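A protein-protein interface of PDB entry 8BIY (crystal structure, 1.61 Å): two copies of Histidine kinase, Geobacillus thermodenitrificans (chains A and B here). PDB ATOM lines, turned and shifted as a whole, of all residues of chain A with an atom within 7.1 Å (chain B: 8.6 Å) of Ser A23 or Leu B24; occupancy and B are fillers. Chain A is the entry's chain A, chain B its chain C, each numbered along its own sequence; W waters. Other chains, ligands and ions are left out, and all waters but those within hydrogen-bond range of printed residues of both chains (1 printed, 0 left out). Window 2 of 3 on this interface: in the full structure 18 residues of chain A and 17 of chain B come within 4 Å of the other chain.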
ATOM      1  N   THR A  18     -25.507 -12.519 -22.844  1.00  0.00           N
ATOM      2  CA  THR A  18     -24.280 -12.321 -22.076  1.00  0.00           C
ATOM      3  C   THR A  18     -23.726 -10.913 -22.284  1.00  0.00           C
ATOM      4  O   THR A  18     -23.350 -10.232 -21.319  1.00  0.00           O
ATOM      5  CB  THR A  18     -23.263 -13.402 -22.443  1.00  0.00           C
ATOM      6  OG1 THR A  18     -23.869 -14.694 -22.276  1.00  0.00           O
ATOM      7  CG2 THR A  18     -22.011 -13.307 -21.555  1.00  0.00           C
ATOM      8  N   VAL A  19     -23.709 -10.443 -23.532  1.00  0.00           N
ATOM      9  CA  VAL A  19     -23.325  -9.061 -23.823  1.00  0.00           C
ATOM     10  C   VAL A  19     -24.225  -8.082 -23.065  1.00  0.00           C
ATOM     11  O   VAL A  19     -23.753  -7.117 -22.451  1.00  0.00           O
ATOM     12  CB  VAL A  19     -23.373  -8.818 -25.348  1.00  0.00           C
ATOM     13  CG1 VAL A  19     -23.184  -7.340 -25.668  1.00  0.00           C
ATOM     14  CG2 VAL A  19     -22.272  -9.609 -26.022  1.00  0.00           C
ATOM     15  N   ALA A  20     -25.542  -8.316 -23.093  1.00  0.00           N
ATOM     16  CA  ALA A  20     -26.477  -7.376 -22.478  1.00  0.00           C
ATOM     17  C   ALA A  20     -26.316  -7.312 -20.963  1.00  0.00           C
ATOM     18  O   ALA A  20     -26.685  -6.303 -20.352  1.00  0.00           O
ATOM     19  CB  ALA A  20     -27.926  -7.756 -22.847  1.00  0.00           C
ATOM     20  N   SER A  21     -25.755  -8.357 -20.354  1.00  0.00           N
ATOM     21  CA  SER A  21     -25.546  -8.435 -18.912  1.00  0.00           C
ATOM     22  C   SER A  21     -24.215  -7.860 -18.454  1.00  0.00           C
ATOM     23  O   SER A  21     -24.007  -7.725 -17.241  1.00  0.00           O
ATOM     24  CB  SER A  21     -25.639  -9.898 -18.448  1.00  0.00           C
ATOM     25  OG  SER A  21     -26.959 -10.378 -18.614  1.00  0.00           O
ATOM     26  N   THR A  22     -23.307  -7.524 -19.365  1.00  0.00           N
ATOM     27  CA  THR A  22     -22.012  -7.009 -18.935  1.00  0.00           C
ATOM     28  C   THR A  22     -22.152  -5.606 -18.375  1.00  0.00           C
ATOM     29  O   THR A  22     -22.959  -4.800 -18.850  1.00  0.00           O
ATOM     30  CB  THR A  22     -21.004  -7.013 -20.081  1.00  0.00           C
ATOM     31  OG1 THR A  22     -21.423  -6.075 -21.078  1.00  0.00           O
ATOM     32  CG2 THR A  22     -20.878  -8.398 -20.688  1.00  0.00           C
ATOM     33  N   SER A  23     -21.362  -5.313 -17.340  1.00  0.00           N
ATOM     34  CA  SER A  23     -21.393  -3.976 -16.760  1.00  0.00           C
ATOM     35  C   SER A  23     -20.989  -2.916 -17.777  1.00  0.00           C
ATOM     36  O   SER A  23     -21.560  -1.821 -17.795  1.00  0.00           O
ATOM     37  CB  SER A  23     -20.494  -3.930 -15.520  1.00  0.00           C
ATOM     38  OG  SER A  23     -19.155  -4.232 -15.853  1.00  0.00           O
ATOM     39  N   LEU A  24     -20.019  -3.222 -18.647  1.00  0.00           N
ATOM     40  CA  LEU A  24     -19.593  -2.238 -19.641  1.00  0.00           C
ATOM     41  C   LEU A  24     -20.769  -1.807 -20.506  1.00  0.00           C
ATOM     42  O   LEU A  24     -20.972  -0.617 -20.763  1.00  0.00           O
ATOM     43  CB  LEU A  24     -18.471  -2.810 -20.520  1.00  0.00           C
ATOM     44  CG  LEU A  24     -17.992  -2.004 -21.742  1.00  0.00           C
ATOM     45  CD1 LEU A  24     -16.513  -2.267 -22.013  1.00  0.00           C
ATOM     46  CD2 LEU A  24     -18.790  -2.272 -23.010  1.00  0.00           C
ATOM     47  N   VAL A  25     -21.553  -2.772 -20.981  1.00  0.00           N
ATOM     48  CA  VAL A  25     -22.627  -2.422 -21.909  1.00  0.00           C
ATOM     49  C   VAL A  25     -23.718  -1.626 -21.210  1.00  0.00           C
ATOM     50  O   VAL A  25     -24.213  -0.627 -21.743  1.00  0.00           O
ATOM     51  CB  VAL A  25     -23.165  -3.694 -22.575  1.00  0.00           C
ATOM     52  CG1 VAL A  25     -24.497  -3.403 -23.296  1.00  0.00           C
ATOM     53  CG2 VAL A  25     -22.097  -4.243 -23.533  1.00  0.00           C
ATOM     54  N   ARG A  26     -24.080  -2.014 -19.988  1.00  0.00           N
ATOM     55  CA  ARG A  26     -25.082  -1.260 -19.244  1.00  0.00           C
ATOM     56  C   ARG A  26     -24.597   0.152 -18.912  1.00  0.00           C
ATOM     57  O   ARG A  26     -25.358   1.121 -19.023  1.00  0.00           O
ATOM     58  CB  ARG A  26     -25.431  -2.041 -17.979  1.00  0.00           C
ATOM     59  CG  ARG A  26     -25.929  -3.443 -18.332  1.00  0.00           C
ATOM     60  CD  ARG A  26     -26.126  -4.323 -17.114  1.00  0.00           C
ATOM     61  NE  ARG A  26     -27.312  -3.924 -16.361  1.00  0.00           N
ATOM     62  CZ  ARG A  26     -27.509  -4.217 -15.085  1.00  0.00           C
ATOM     63  NH1 ARG A  26     -26.652  -4.964 -14.409  1.00  0.00           N
ATOM     64  NH2 ARG A  26     -28.589  -3.742 -14.470  1.00  0.00           N
ATOM     65  N   GLU A  27     -23.327   0.289 -18.525  1.00  0.00           N
ATOM     66  CA  GLU A  27     -22.766   1.594 -18.158  1.00  0.00           C
ATOM     67  C   GLU A  27     -22.636   2.515 -19.363  1.00  0.00           C
ATOM     68  O   GLU A  27     -22.821   3.729 -19.245  1.00  0.00           O
ATOM     69  CB  GLU A  27     -21.386   1.409 -17.535  1.00  0.00           C
ATOM     70  CG  GLU A  27     -21.349   0.795 -16.154  1.00  0.00           C
ATOM     71  CD  GLU A  27     -19.934   0.505 -15.680  1.00  0.00           C
ATOM     72  OE1 GLU A  27     -18.944   0.759 -16.422  1.00  0.00           O
ATOM     73  OE2 GLU A  27     -19.813  -0.009 -14.556  1.00  0.00           O
ATOM     74  N   ALA A  28     -22.255   1.967 -20.521  1.00  0.00           N
ATOM     75  CA  ALA A  28     -21.955   2.807 -21.678  1.00  0.00           C
ATOM     76  C   ALA A  28     -23.149   3.638 -22.118  1.00  0.00           C
ATOM     77  O   ALA A  28     -22.988   4.700 -22.733  1.00  0.00           O
ATOM     78  CB  ALA A  28     -21.467   1.934 -22.839  1.00  0.00           C
ATOM     79  N   PHE A  29     -24.364   3.182 -21.834  1.00  0.00           N
ATOM     80  CA  PHE A  29     -25.520   3.943 -22.265  1.00  0.00           C
ATOM     81  C   PHE A  29     -25.647   5.286 -21.554  1.00  0.00           C
ATOM     82  O   PHE A  29     -26.411   6.146 -22.009  1.00  0.00           O
ATOM     83  CB  PHE A  29     -26.756   3.067 -22.072  1.00  0.00           C
ATOM     84  CG  PHE A  29     -27.002   2.154 -23.233  1.00  0.00           C
ATOM     85  CD1 PHE A  29     -26.283   0.981 -23.378  1.00  0.00           C
ATOM     86  CD2 PHE A  29     -27.932   2.488 -24.190  1.00  0.00           C
ATOM     87  CE1 PHE A  29     -26.495   0.158 -24.459  1.00  0.00           C
ATOM     88  CE2 PHE A  29     -28.150   1.662 -25.277  1.00  0.00           C
ATOM     89  CZ  PHE A  29     -27.423   0.505 -25.417  1.00  0.00           C
ATOM     90  N   ARG A  37     -17.163   3.173 -26.122  1.00  0.00           N
ATOM     91  CA  ARG A  37     -16.971   1.940 -25.369  1.00  0.00           C
ATOM     92  C   ARG A  37     -17.685   0.736 -25.976  1.00  0.00           C
ATOM     93  O   ARG A  37     -17.168  -0.383 -25.892  1.00  0.00           O
ATOM     94  CB  ARG A  37     -17.455   2.139 -23.935  1.00  0.00           C
ATOM     95  CG  ARG A  37     -16.489   2.932 -23.099  1.00  0.00           C
ATOM     96  CD  ARG A  37     -16.592   2.538 -21.649  1.00  0.00           C
ATOM     97  NE  ARG A  37     -17.734   3.195 -21.041  1.00  0.00           N
ATOM     98  CZ  ARG A  37     -18.218   2.942 -19.831  1.00  0.00           C
ATOM     99  NH1 ARG A  37     -17.670   2.038 -19.033  1.00  0.00           N
ATOM    100  NH2 ARG A  37     -19.271   3.623 -19.407  1.00  0.00           N
ATOM    101  N   THR B  18     -17.250 -15.079 -24.442  1.00  0.00           N
ATOM    102  CA  THR B  18     -17.814 -13.774 -24.107  1.00  0.00           C
ATOM    103  C   THR B  18     -17.540 -13.412 -22.651  1.00  0.00           C
ATOM    104  O   THR B  18     -17.134 -12.282 -22.354  1.00  0.00           O
ATOM    105  CB  THR B  18     -19.310 -13.745 -24.411  1.00  0.00           C
ATOM    106  OG1 THR B  18     -19.522 -14.122 -25.778  1.00  0.00           O
ATOM    107  CG2 THR B  18     -19.878 -12.333 -24.204  1.00  0.00           C
ATOM    108  N   VAL B  19     -17.718 -14.368 -21.732  1.00  0.00           N
ATOM    109  CA  VAL B  19     -17.410 -14.113 -20.325  1.00  0.00           C
ATOM    110  C   VAL B  19     -15.926 -13.791 -20.163  1.00  0.00           C
ATOM    111  O   VAL B  19     -15.552 -12.843 -19.462  1.00  0.00           O
ATOM    112  CB  VAL B  19     -17.825 -15.323 -19.468  1.00  0.00           C
ATOM    113  CG1 VAL B  19     -17.334 -15.164 -18.002  1.00  0.00           C
ATOM    114  CG2 VAL B  19     -19.329 -15.508 -19.494  1.00  0.00           C
ATOM    115  N   ALA B  20     -15.064 -14.561 -20.839  1.00  0.00           N
ATOM    116  CA  ALA B  20     -13.615 -14.373 -20.704  1.00  0.00           C
ATOM    117  C   ALA B  20     -13.160 -13.003 -21.208  1.00  0.00           C
ATOM    118  O   ALA B  20     -12.097 -12.512 -20.797  1.00  0.00           O
ATOM    119  CB  ALA B  20     -12.868 -15.476 -21.449  1.00  0.00           C
ATOM    120  N   SER B  21     -13.905 -12.411 -22.146  1.00  0.00           N
ATOM    121  CA  SER B  21     -13.566 -11.122 -22.738  1.00  0.00           C
ATOM    122  C   SER B  21     -14.205  -9.947 -22.013  1.00  0.00           C
ATOM    123  O   SER B  21     -13.944  -8.796 -22.379  1.00  0.00           O
ATOM    124  CB  SER B  21     -13.989 -11.083 -24.215  1.00  0.00           C
ATOM    125  OG  SER B  21     -13.281 -12.052 -24.968  1.00  0.00           O
ATOM    126  N   THR B  22     -15.026 -10.203 -20.998  1.00  0.00           N
ATOM    127  CA  THR B  22     -15.677  -9.124 -20.270  1.00  0.00           C
ATOM    128  C   THR B  22     -14.665  -8.428 -19.366  1.00  0.00           C
ATOM    129  O   THR B  22     -13.878  -9.083 -18.680  1.00  0.00           O
ATOM    130  CB  THR B  22     -16.850  -9.671 -19.451  1.00  0.00           C
ATOM    131  OG1 THR B  22     -17.803 -10.282 -20.326  1.00  0.00           O
ATOM    132  CG2 THR B  22     -17.555  -8.567 -18.697  1.00  0.00           C
ATOM    133  N   SER B  23     -14.676  -7.094 -19.380  1.00  0.00           N
ATOM    134  CA  SER B  23     -13.721  -6.341 -18.574  1.00  0.00           C
ATOM    135  C   SER B  23     -13.857  -6.683 -17.097  1.00  0.00           C
ATOM    136  O   SER B  23     -12.855  -6.768 -16.377  1.00  0.00           O
ATOM    137  CB  SER B  23     -13.929  -4.850 -18.802  1.00  0.00           C
ATOM    138  OG  SER B  23     -15.289  -4.538 -18.586  1.00  0.00           O
ATOM    139  N   LEU B  24     -15.091  -6.887 -16.629  1.00  0.00           N
ATOM    140  CA  LEU B  24     -15.319  -7.233 -15.225  1.00  0.00           C
ATOM    141  C   LEU B  24     -14.499  -8.439 -14.803  1.00  0.00           C
ATOM    142  O   LEU B  24     -13.941  -8.475 -13.701  1.00  0.00           O
ATOM    143  CB  LEU B  24     -16.815  -7.511 -15.012  1.00  0.00           C
ATOM    144  CG  LEU B  24     -17.374  -7.829 -13.624  1.00  0.00           C
ATOM    145  CD1 LEU B  24     -18.846  -7.499 -13.603  1.00  0.00           C
ATOM    146  CD2 LEU B  24     -17.200  -9.304 -13.313  1.00  0.00           C
ATOM    147  N   VAL B  25     -14.422  -9.438 -15.671  1.00  0.00           N
ATOM    148  CA  VAL B  25     -13.788 -10.694 -15.309  1.00  0.00           C
ATOM    149  C   VAL B  25     -12.279 -10.514 -15.232  1.00  0.00           C
ATOM    150  O   VAL B  25     -11.636 -10.905 -14.253  1.00  0.00           O
ATOM    151  CB  VAL B  25     -14.188 -11.775 -16.322  1.00  0.00           C
ATOM    152  CG1 VAL B  25     -13.326 -13.026 -16.176  1.00  0.00           C
ATOM    153  CG2 VAL B  25     -15.669 -12.086 -16.183  1.00  0.00           C
ATOM    154  N   ARG B  26     -11.701  -9.896 -16.262  1.00  0.00           N
ATOM    155  CA  ARG B  26     -10.263  -9.643 -16.290  1.00  0.00           C
ATOM    156  C   ARG B  26      -9.832  -8.787 -15.103  1.00  0.00           C
ATOM    157  O   ARG B  26      -8.819  -9.073 -14.451  1.00  0.00           O
ATOM    158  CB  ARG B  26      -9.922  -8.986 -17.630  1.00  0.00           C
ATOM    159  CG  ARG B  26     -10.439  -9.842 -18.799  1.00  0.00           C
ATOM    160  CD  ARG B  26     -10.277  -9.223 -20.181  1.00  0.00           C
ATOM    161  NE  ARG B  26      -8.888  -9.009 -20.568  1.00  0.00           N
ATOM    162  CZ  ARG B  26      -8.517  -8.329 -21.644  1.00  0.00           C
ATOM    163  NH1 ARG B  26      -9.407  -7.790 -22.461  1.00  0.00           N
ATOM    164  NH2 ARG B  26      -7.221  -8.192 -21.910  1.00  0.00           N
ATOM    165  N   GLU B  27     -10.623  -7.763 -14.776  1.00  0.00           N
ATOM    166  CA  GLU B  27     -10.303  -6.853 -13.681  1.00  0.00           C
ATOM    167  C   GLU B  27     -10.384  -7.540 -12.322  1.00  0.00           C
ATOM    168  O   GLU B  27      -9.611  -7.217 -11.412  1.00  0.00           O
ATOM    169  CB  GLU B  27     -11.260  -5.667 -13.724  1.00  0.00           C
ATOM    170  CG  GLU B  27     -11.075  -4.734 -14.904  1.00  0.00           C
ATOM    171  CD  GLU B  27     -12.226  -3.750 -15.037  1.00  0.00           C
ATOM    172  OE1 GLU B  27     -12.920  -3.496 -14.029  1.00  0.00           O
ATOM    173  OE2 GLU B  27     -12.451  -3.250 -16.158  1.00  0.00           O
ATOM    174  N   ALA B  28     -11.334  -8.464 -12.153  1.00  0.00           N
ATOM    175  CA  ALA B  28     -11.505  -9.105 -10.849  1.00  0.00           C
ATOM    176  C   ALA B  28     -10.260  -9.868 -10.421  1.00  0.00           C
ATOM    177  O   ALA B  28     -10.052 -10.090  -9.222  1.00  0.00           O
ATOM    178  CB  ALA B  28     -12.703 -10.051 -10.872  1.00  0.00           C
ATOM    179  N   PHE B  29      -9.440 -10.304 -11.373  1.00  0.00           N
ATOM    180  CA  PHE B  29      -8.232 -11.043 -11.028  1.00  0.00           C
ATOM    181  C   PHE B  29      -7.185 -10.174 -10.341  1.00  0.00           C
ATOM    182  O   PHE B  29      -6.242 -10.720  -9.760  1.00  0.00           O
ATOM    183  CB  PHE B  29      -7.655 -11.713 -12.278  1.00  0.00           C
ATOM    184  CG  PHE B  29      -8.301 -13.033 -12.606  1.00  0.00           C
ATOM    185  CD1 PHE B  29      -9.590 -13.082 -13.108  1.00  0.00           C
ATOM    186  CD2 PHE B  29      -7.629 -14.225 -12.400  1.00  0.00           C
ATOM    187  CE1 PHE B  29     -10.192 -14.299 -13.400  1.00  0.00           C
ATOM    188  CE2 PHE B  29      -8.222 -15.441 -12.699  1.00  0.00           C
ATOM    189  CZ  PHE B  29      -9.509 -15.476 -13.198  1.00  0.00           C
ATOM    190  N   ARG B  30      -7.338  -8.848 -10.369  1.00  0.00           N
ATOM    191  CA  ARG B  30      -6.474  -7.958  -9.598  1.00  0.00           C
ATOM    192  C   ARG B  30      -6.933  -7.796  -8.154  1.00  0.00           C
ATOM    193  O   ARG B  30      -6.180  -7.244  -7.342  1.00  0.00           O
ATOM    194  CB  ARG B  30      -6.404  -6.577 -10.257  1.00  0.00           C
ATOM    195  CG  ARG B  30      -5.860  -6.577 -11.673  1.00  0.00           C
ATOM    196  N   ASP B  31      -8.144  -8.240  -7.821  1.00  0.00           N
ATOM    197  CA  ASP B  31      -8.670  -8.136  -6.466  1.00  0.00           C
ATOM    198  C   ASP B  31      -8.047  -9.195  -5.564  1.00  0.00           C
ATOM    199  O   ASP B  31      -7.629 -10.261  -6.022  1.00  0.00           O
ATOM    200  CB  ASP B  31     -10.192  -8.308  -6.453  1.00  0.00           C
ATOM    201  CG  ASP B  31     -10.908  -7.260  -7.275  1.00  0.00           C
ATOM    202  OD1 ASP B  31     -10.298  -6.203  -7.546  1.00  0.00           O
ATOM    203  OD2 ASP B  31     -12.082  -7.489  -7.643  1.00  0.00           O
ATOM    204  N   PRO B  34     -10.986 -12.337  -5.865  1.00  0.00           N
ATOM    205  CA  PRO B  34     -11.720 -12.205  -7.139  1.00  0.00           C
ATOM    206  C   PRO B  34     -13.147 -12.738  -7.101  1.00  0.00           C
ATOM    207  O   PRO B  34     -13.963 -12.305  -7.921  1.00  0.00           O
ATOM    208  CB  PRO B  34     -10.861 -13.013  -8.117  1.00  0.00           C
ATOM    209  CG  PRO B  34      -9.467 -12.969  -7.517  1.00  0.00           C
ATOM    210  CD  PRO B  34      -9.712 -13.055  -6.035  1.00  0.00           C
ATOM    211  N   SER B  35     -13.475 -13.659  -6.186  1.00  0.00           N
ATOM    212  CA  SER B  35     -14.816 -14.243  -6.166  1.00  0.00           C
ATOM    213  C   SER B  35     -15.894 -13.209  -5.891  1.00  0.00           C
ATOM    214  O   SER B  35     -17.045 -13.390  -6.310  1.00  0.00           O
ATOM    215  CB  SER B  35     -14.907 -15.358  -5.128  1.00  0.00           C
ATOM    216  OG  SER B  35     -13.969 -16.372  -5.409  1.00  0.00           O
ATOM    217  N   VAL B  36     -15.566 -12.128  -5.181  1.00  0.00           N
ATOM    218  CA  VAL B  36     -16.602 -11.164  -4.823  1.00  0.00           C
ATOM    219  C   VAL B  36     -17.265 -10.602  -6.071  1.00  0.00           C
ATOM    220  O   VAL B  36     -18.494 -10.466  -6.132  1.00  0.00           O
ATOM    221  CB  VAL B  36     -16.018 -10.051  -3.932  1.00  0.00           C
ATOM    222  CG1 VAL B  36     -17.101  -9.052  -3.566  1.00  0.00           C
ATOM    223  CG2 VAL B  36     -15.390 -10.654  -2.675  1.00  0.00           C
ATOM    224  N   ARG B  37     -16.475 -10.295  -7.098  1.00  0.00           N
ATOM    225  CA  ARG B  37     -17.060  -9.810  -8.339  1.00  0.00           C
ATOM    226  C   ARG B  37     -17.368 -10.933  -9.320  1.00  0.00           C
ATOM    227  O   ARG B  37     -18.349 -10.827 -10.070  1.00  0.00           O
ATOM    228  CB  ARG B  37     -16.136  -8.786  -9.011  1.00  0.00           C
ATOM    229  CG  ARG B  37     -16.127  -7.410  -8.357  1.00  0.00           C
ATOM    230  N   LEU B  38     -16.568 -12.006  -9.320  1.00  0.00           N
ATOM    231  CA  LEU B  38     -16.731 -13.038 -10.341  1.00  0.00           C
ATOM    232  C   LEU B  38     -17.992 -13.866 -10.118  1.00  0.00           C
ATOM    233  O   LEU B  38     -18.693 -14.196 -11.082  1.00  0.00           O
ATOM    234  CB  LEU B  38     -15.514 -13.951 -10.396  1.00  0.00           C
ATOM    235  CG  LEU B  38     -14.222 -13.335 -10.939  1.00  0.00           C
ATOM    236  CD1 LEU B  38     -13.079 -14.329 -10.836  1.00  0.00           C
ATOM    237  CD2 LEU B  38     -14.440 -12.910 -12.392  1.00  0.00           C
ATOM    238  N   GLN B  39     -18.290 -14.231  -8.867  1.00  0.00           N
ATOM    239  CA  GLN B  39     -19.405 -15.148  -8.613  1.00  0.00           C
ATOM    240  C   GLN B  39     -20.768 -14.565  -8.987  1.00  0.00           C
ATOM    241  O   GLN B  39     -21.555 -15.279  -9.631  1.00  0.00           O
ATOM    242  CB  GLN B  39     -19.370 -15.621  -7.155  1.00  0.00           C
ATOM    243  CG  GLN B  39     -20.563 -16.477  -6.739  1.00  0.00           C
ATOM    244  CD  GLN B  39     -20.597 -17.824  -7.448  1.00  0.00           C
ATOM    245  OE1 GLN B  39     -19.616 -18.243  -8.069  1.00  0.00           O
ATOM    246  NE2 GLN B  39     -21.742 -18.498  -7.378  1.00  0.00           N
ATOM    247  N   PRO B  40     -21.125 -13.319  -8.638  1.00  0.00           N
ATOM    248  CA  PRO B  40     -22.439 -12.811  -9.074  1.00  0.00           C
ATOM    249  C   PRO B  40     -22.573 -12.701 -10.581  1.00  0.00           C
ATOM    250  O   PRO B  40     -23.666 -12.922 -11.118  1.00  0.00           O
ATOM    251  CB  PRO B  40     -22.549 -11.429  -8.407  1.00  0.00           C
ATOM    252  CG  PRO B  40     -21.433 -11.327  -7.461  1.00  0.00           C
ATOM    253  CD  PRO B  40     -20.436 -12.397  -7.709  1.00  0.00           C
ATOM    254  N   PHE B  41     -21.494 -12.352 -11.280  1.00  0.00           N
ATOM    255  CA  PHE B  41     -21.575 -12.250 -12.730  1.00  0.00           C
ATOM    256  C   PHE B  41     -21.727 -13.623 -13.356  1.00  0.00           C
ATOM    257  O   PHE B  41     -22.597 -13.830 -14.218  1.00  0.00           O
ATOM    258  CB  PHE B  41     -20.344 -11.537 -13.286  1.00  0.00           C
ATOM    259  CG  PHE B  41     -20.378 -11.387 -14.779  1.00  0.00           C
ATOM    260  CD1 PHE B  41     -21.398 -10.668 -15.397  1.00  0.00           C
ATOM    261  CD2 PHE B  41     -19.407 -11.976 -15.562  1.00  0.00           C
ATOM    262  CE1 PHE B  41     -21.447 -10.550 -16.792  1.00  0.00           C
ATOM    263  CE2 PHE B  41     -19.431 -11.858 -16.957  1.00  0.00           C
ATOM    264  CZ  PHE B  41     -20.455 -11.138 -17.569  1.00  0.00           C
ATOM    265  N   ALA B  42     -20.890 -14.574 -12.930  1.00  0.00           N
ATOM    266  CA  ALA B  42     -20.980 -15.939 -13.443  1.00  0.00           C
ATOM    267  C   ALA B  42     -22.367 -16.514 -13.213  1.00  0.00           C
ATOM    268  O   ALA B  42     -22.939 -17.147 -14.110  1.00  0.00           O
ATOM    269  CB  ALA B  42     -19.918 -16.820 -12.785  1.00  0.00           C
ATOM    270  N   ILE B  45     -24.876 -14.958 -15.612  1.00  0.00           N
ATOM    271  CA  ILE B  45     -24.749 -15.500 -16.963  1.00  0.00           C
ATOM    272  C   ILE B  45     -25.267 -16.930 -17.019  1.00  0.00           C
ATOM    273  O   ILE B  45     -25.928 -17.324 -17.987  1.00  0.00           O
ATOM    274  CB  ILE B  45     -23.294 -15.409 -17.459  1.00  0.00           C
ATOM    275  CG1 ILE B  45     -22.843 -13.946 -17.512  1.00  0.00           C
ATOM    276  CG2 ILE B  45     -23.142 -16.106 -18.832  1.00  0.00           C
ATOM    277  CD1 ILE B  45     -23.875 -13.025 -18.223  1.00  0.00           C
ATOM    278  N   ILE B  56     -15.281 -20.017 -13.354  1.00  0.00           N
ATOM    279  CA  ILE B  56     -14.153 -19.154 -13.663  1.00  0.00           C
ATOM    280  C   ILE B  56     -13.045 -19.494 -12.678  1.00  0.00           C
ATOM    281  O   ILE B  56     -13.268 -19.477 -11.466  1.00  0.00           O
ATOM    282  CB  ILE B  56     -14.530 -17.666 -13.584  1.00  0.00           C
ATOM    283  CG1 ILE B  56     -15.770 -17.397 -14.452  1.00  0.00           C
ATOM    284  CG2 ILE B  56     -13.356 -16.802 -14.011  1.00  0.00           C
ATOM    285  CD1 ILE B  56     -16.357 -16.019 -14.299  1.00  0.00           C
ATOM    286  N   ILE B 108      -8.629 -16.592 -20.187  1.00  0.00           N
ATOM    287  CA  ILE B 108      -8.711 -15.194 -19.781  1.00  0.00           C
ATOM    288  C   ILE B 108      -7.333 -14.568 -19.919  1.00  0.00           C
ATOM    289  O   ILE B 108      -6.363 -15.063 -19.331  1.00  0.00           O
ATOM    290  CB  ILE B 108      -9.229 -15.045 -18.341  1.00  0.00           C
ATOM    291  CG1 ILE B 108     -10.526 -15.850 -18.152  1.00  0.00           C
ATOM    292  CG2 ILE B 108      -9.418 -13.581 -18.003  1.00  0.00           C
ATOM    293  CD1 ILE B 108     -10.965 -15.951 -16.694  1.00  0.00           C
HETATM  294  O   HOH W   1     -17.824  -5.442 -18.189  1.00  0.00           O
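Water W1 lies within hydrogen-bond range of OG of Ser B23, OG of Ser A23, N of Leu A24 and N of Leu B24.
Hydrophobic or aromatic side chains of chain B that line the printed part of chain A: Leu B24, Phe B41 and Ile B45. Among the printed residues, 6 pairs touch across the chains. Among the printed residues, no Asp or Glu carboxylate lies within 4 Å of a Lys or Arg side-chain nitrogen of the other chain.
Of the printed residues of chain B, Thr A22 touches Thr B22. Printed residues of chain B within 4 Å of Ser A23: Leu B24 (3.98 Å). Printed residues of chain A within 4 Å of Leu B24: Ser A23 (3.98 Å). Of the printed residues of chain A, Phe B41 touches Ser A21 (3.8 Å). The nearest printed residue of chain B that does not touch Ser A23 is Ser B23 (4.7 Å). The nearest printed residue of chain A that does not touch Leu B24 is Thr A22 (6.1 Å). The nearest printed residue of chain B that does not touch Thr A18 is Val B19 (4.04 Å).
OG1 of Thr A22 sits at hydrogen-bond distance from O of Val A19, 2.9 Å away. OG1 of Thr A22 sits close to N of Val A25, 3.3 Å away. The side-chain hydroxyl (OG1) of Thr B22 is in hydrogen-bond range of the backbone carbonyl oxygen (O) of Thr B18 (2.9 Å).
Among the printed residues, pairs that only touch across the chains: Thr A18 with Thr B18, Ser A21 with Ile B45, Thr A22 with Thr B22, Thr A18 with Ile B45, Ser A21 with Phe B41 and Ser A23 with Leu B24.
Thr B18 touches its own counterpart, Thr A18. Thr A22 touches its own counterpart, Thr B22. Ser A23 touches Leu B24, but with the chains exchanged Leu A24 does not touch Ser B23 (4.1 Å). Of the 6 pairs that touch across the chains among the printed residues, 2 have their exchanged pair printed and touching as well.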
